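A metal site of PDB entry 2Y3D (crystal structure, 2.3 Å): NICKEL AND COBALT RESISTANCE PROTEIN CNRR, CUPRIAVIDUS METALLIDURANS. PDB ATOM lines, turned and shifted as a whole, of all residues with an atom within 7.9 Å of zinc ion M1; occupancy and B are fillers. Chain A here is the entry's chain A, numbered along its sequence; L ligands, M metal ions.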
ATOM      1  N   HIS A  12     -19.752  16.737  -0.108  1.00  0.00           N
ATOM      2  CA  HIS A  12     -21.138  17.110  -0.235  1.00  0.00           C
ATOM      3  C   HIS A  12     -21.398  18.349   0.615  1.00  0.00           C
ATOM      4  O   HIS A  12     -22.143  19.238   0.214  1.00  0.00           O
ATOM      5  CB  HIS A  12     -22.051  15.954   0.191  1.00  0.00           C
ATOM      6  CG  HIS A  12     -23.481  16.130  -0.224  1.00  0.00           C
ATOM      7  ND1 HIS A  12     -23.893  15.985  -1.526  1.00  0.00           N
ATOM      8  CD2 HIS A  12     -24.573  16.471   0.497  1.00  0.00           C
ATOM      9  CE1 HIS A  12     -25.195  16.219  -1.589  1.00  0.00           C
ATOM     10  NE2 HIS A  12     -25.630  16.507  -0.385  1.00  0.00           N
ATOM     11  N   GLU A  13     -20.766  18.420   1.780  1.00  0.00           N
ATOM     12  CA  GLU A  13     -20.885  19.615   2.612  1.00  0.00           C
ATOM     13  C   GLU A  13     -20.356  20.821   1.845  1.00  0.00           C
ATOM     14  O   GLU A  13     -20.986  21.877   1.825  1.00  0.00           O
ATOM     15  CB  GLU A  13     -20.166  19.416   3.934  1.00  0.00           C
ATOM     16  CG  GLU A  13     -20.951  18.511   4.870  1.00  0.00           C
ATOM     17  CD  GLU A  13     -22.412  18.915   4.947  1.00  0.00           C
ATOM     18  OE1 GLU A  13     -22.673  20.115   5.209  1.00  0.00           O
ATOM     19  OE2 GLU A  13     -23.291  18.046   4.742  1.00  0.00           O
ATOM     20  N   LEU A  15     -20.601  21.143  -1.052  1.00  0.00           N
ATOM     21  CA  LEU A  15     -21.726  21.428  -1.944  1.00  0.00           C
ATOM     22  C   LEU A  15     -22.835  22.189  -1.222  1.00  0.00           C
ATOM     23  O   LEU A  15     -23.351  23.178  -1.738  1.00  0.00           O
ATOM     24  CB  LEU A  15     -22.260  20.145  -2.582  1.00  0.00           C
ATOM     25  CG  LEU A  15     -21.788  19.757  -3.988  1.00  0.00           C
ATOM     26  CD1 LEU A  15     -20.631  20.622  -4.486  1.00  0.00           C
ATOM     27  CD2 LEU A  15     -21.425  18.276  -4.061  1.00  0.00           C
ATOM     28  N   HIS A  16     -23.213  21.732  -0.027  1.00  0.00           N
ATOM     29  CA  HIS A  16     -24.217  22.425   0.783  1.00  0.00           C
ATOM     30  C   HIS A  16     -23.829  23.899   0.991  1.00  0.00           C
ATOM     31  O   HIS A  16     -24.692  24.741   1.272  1.00  0.00           O
ATOM     32  CB  HIS A  16     -24.361  21.754   2.164  1.00  0.00           C
ATOM     33  CG  HIS A  16     -25.357  20.629   2.204  1.00  0.00           C
ATOM     34  ND1 HIS A  16     -25.624  19.918   3.346  1.00  0.00           N
ATOM     35  CD2 HIS A  16     -26.144  20.094   1.239  1.00  0.00           C
ATOM     36  CE1 HIS A  16     -26.537  18.993   3.094  1.00  0.00           C
ATOM     37  NE2 HIS A  16     -26.871  19.080   1.819  1.00  0.00           N
ATOM     38  N   LEU A  21     -29.029  27.257  -0.967  1.00  0.00           N
ATOM     39  CA  LEU A  21     -30.343  26.618  -1.008  1.00  0.00           C
ATOM     40  C   LEU A  21     -31.399  27.502  -1.648  1.00  0.00           C
ATOM     41  O   LEU A  21     -32.527  27.103  -1.825  1.00  0.00           O
ATOM     42  CB  LEU A  21     -30.797  26.248   0.380  1.00  0.00           C
ATOM     43  CG  LEU A  21     -30.556  24.783   0.682  1.00  0.00           C
ATOM     44  CD1 LEU A  21     -29.142  24.353   0.287  1.00  0.00           C
ATOM     45  CD2 LEU A  21     -30.852  24.501   2.142  1.00  0.00           C
ATOM     46  N   ARG A  26     -29.465  23.475  -6.415  1.00  0.00           N
ATOM     47  CA  ARG A  26     -29.662  22.666  -5.243  1.00  0.00           C
ATOM     48  C   ARG A  26     -30.549  21.491  -5.506  1.00  0.00           C
ATOM     49  O   ARG A  26     -30.223  20.393  -5.198  1.00  0.00           O
ATOM     50  CB  ARG A  26     -30.269  23.464  -4.121  1.00  0.00           C
ATOM     51  CG  ARG A  26     -30.499  22.630  -2.866  1.00  0.00           C
ATOM     52  CD  ARG A  26     -31.876  22.816  -2.257  1.00  0.00           C
ATOM     53  NE  ARG A  26     -32.700  21.625  -2.344  1.00  0.00           N
ATOM     54  CZ  ARG A  26     -33.836  21.556  -3.025  1.00  0.00           C
ATOM     55  NH1 ARG A  26     -34.274  22.611  -3.683  1.00  0.00           N
ATOM     56  NH2 ARG A  26     -34.528  20.452  -3.056  1.00  0.00           N
ATOM     57  N   LEU A  29     -28.657  19.082  -7.711  1.00  0.00           N
ATOM     58  CA  LEU A  29     -27.668  18.456  -6.866  1.00  0.00           C
ATOM     59  C   LEU A  29     -28.274  17.322  -6.031  1.00  0.00           C
ATOM     60  O   LEU A  29     -27.772  16.186  -6.048  1.00  0.00           O
ATOM     61  CB  LEU A  29     -27.014  19.526  -6.003  1.00  0.00           C
ATOM     62  CG  LEU A  29     -26.005  19.227  -4.923  1.00  0.00           C
ATOM     63  CD1 LEU A  29     -25.200  20.504  -4.678  1.00  0.00           C
ATOM     64  CD2 LEU A  29     -26.708  18.798  -3.659  1.00  0.00           C
ATOM     65  N   GLU A  30     -29.382  17.599  -5.337  1.00  0.00           N
ATOM     66  CA  GLU A  30     -29.963  16.582  -4.474  1.00  0.00           C
ATOM     67  C   GLU A  30     -30.577  15.393  -5.216  1.00  0.00           C
ATOM     68  O   GLU A  30     -30.664  14.296  -4.653  1.00  0.00           O
ATOM     69  CB  GLU A  30     -30.980  17.178  -3.494  1.00  0.00           C
ATOM     70  CG  GLU A  30     -30.393  18.174  -2.509  1.00  0.00           C
ATOM     71  CD  GLU A  30     -29.313  17.594  -1.616  1.00  0.00           C
ATOM     72  OE1 GLU A  30     -29.126  16.349  -1.570  1.00  0.00           O
ATOM     73  OE2 GLU A  30     -28.655  18.411  -0.955  1.00  0.00           O
ATOM     74  N   GLU A  33     -27.751  13.210  -5.916  1.00  0.00           N
ATOM     75  CA  GLU A  33     -27.404  12.562  -4.675  1.00  0.00           C
ATOM     76  C   GLU A  33     -28.337  11.398  -4.395  1.00  0.00           C
ATOM     77  O   GLU A  33     -27.874  10.342  -3.972  1.00  0.00           O
ATOM     78  CB  GLU A  33     -27.421  13.552  -3.508  1.00  0.00           C
ATOM     79  CG  GLU A  33     -26.886  12.951  -2.210  1.00  0.00           C
ATOM     80  CD  GLU A  33     -25.395  12.640  -2.263  1.00  0.00           C
ATOM     81  OE1 GLU A  33     -24.679  13.299  -3.035  1.00  0.00           O
ATOM     82  OE2 GLU A  33     -24.926  11.759  -1.523  1.00  0.00           O
ATOM     83  N   ASP A  34     -29.641  11.584  -4.615  1.00  0.00           N
ATOM     84  CA  ASP A  34     -30.607  10.506  -4.424  1.00  0.00           C
ATOM     85  C   ASP A  34     -30.178   9.290  -5.237  1.00  0.00           C
ATOM     86  O   ASP A  34     -30.230   8.165  -4.738  1.00  0.00           O
ATOM     87  CB  ASP A  34     -32.020  10.884  -4.886  1.00  0.00           C
ATOM     88  CG  ASP A  34     -32.636  12.018  -4.085  1.00  0.00           C
ATOM     89  OD1 ASP A  34     -32.188  12.270  -2.952  1.00  0.00           O
ATOM     90  OD2 ASP A  34     -33.589  12.631  -4.594  1.00  0.00           O
ATOM     91  N   MET A  93     -20.447  15.441  -9.760  1.00  0.00           N
ATOM     92  CA  MET A  93     -20.876  16.530  -8.901  1.00  0.00           C
ATOM     93  C   MET A  93     -19.986  17.743  -9.123  1.00  0.00           C
ATOM     94  O   MET A  93     -20.458  18.872  -9.067  1.00  0.00           O
ATOM     95  CB  MET A  93     -20.881  16.135  -7.426  1.00  0.00           C
ATOM     96  CG  MET A  93     -21.838  15.013  -7.068  1.00  0.00           C
ATOM     97  SD  MET A  93     -23.505  15.171  -7.747  1.00  0.00           S
ATOM     98  CE  MET A  93     -24.221  16.302  -6.537  1.00  0.00           C
HETATM   99 CL1  LIG L   1     -28.628  15.855   1.560  1.00  0.00          CL
HETATM  100 ZN    ZN M   1     -27.388  17.469   0.433  1.00  0.00          ZN
HETATM  101 ZN    ZN M   2     -22.666  12.772  -3.311  1.00  0.00          ZN
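A ring nitrogen (ND1) of His 12 sits close to the side-chain carboxylate (OE1) of Glu 33 (3.2 Å). OE2 of Glu 13 sits at hydrogen-bond distance from ND1 of His 16 (3.3 Å).
Zinc ion M1 is bound by the side-chain carboxylate (OE2) of Glu 30, a ring nitrogen (NE2) of His 12, a ring nitrogen (NE2) of His 16 and a chlorine (CL1) of the ligand. Zinc ion M1 has four donor atoms within binding distance.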
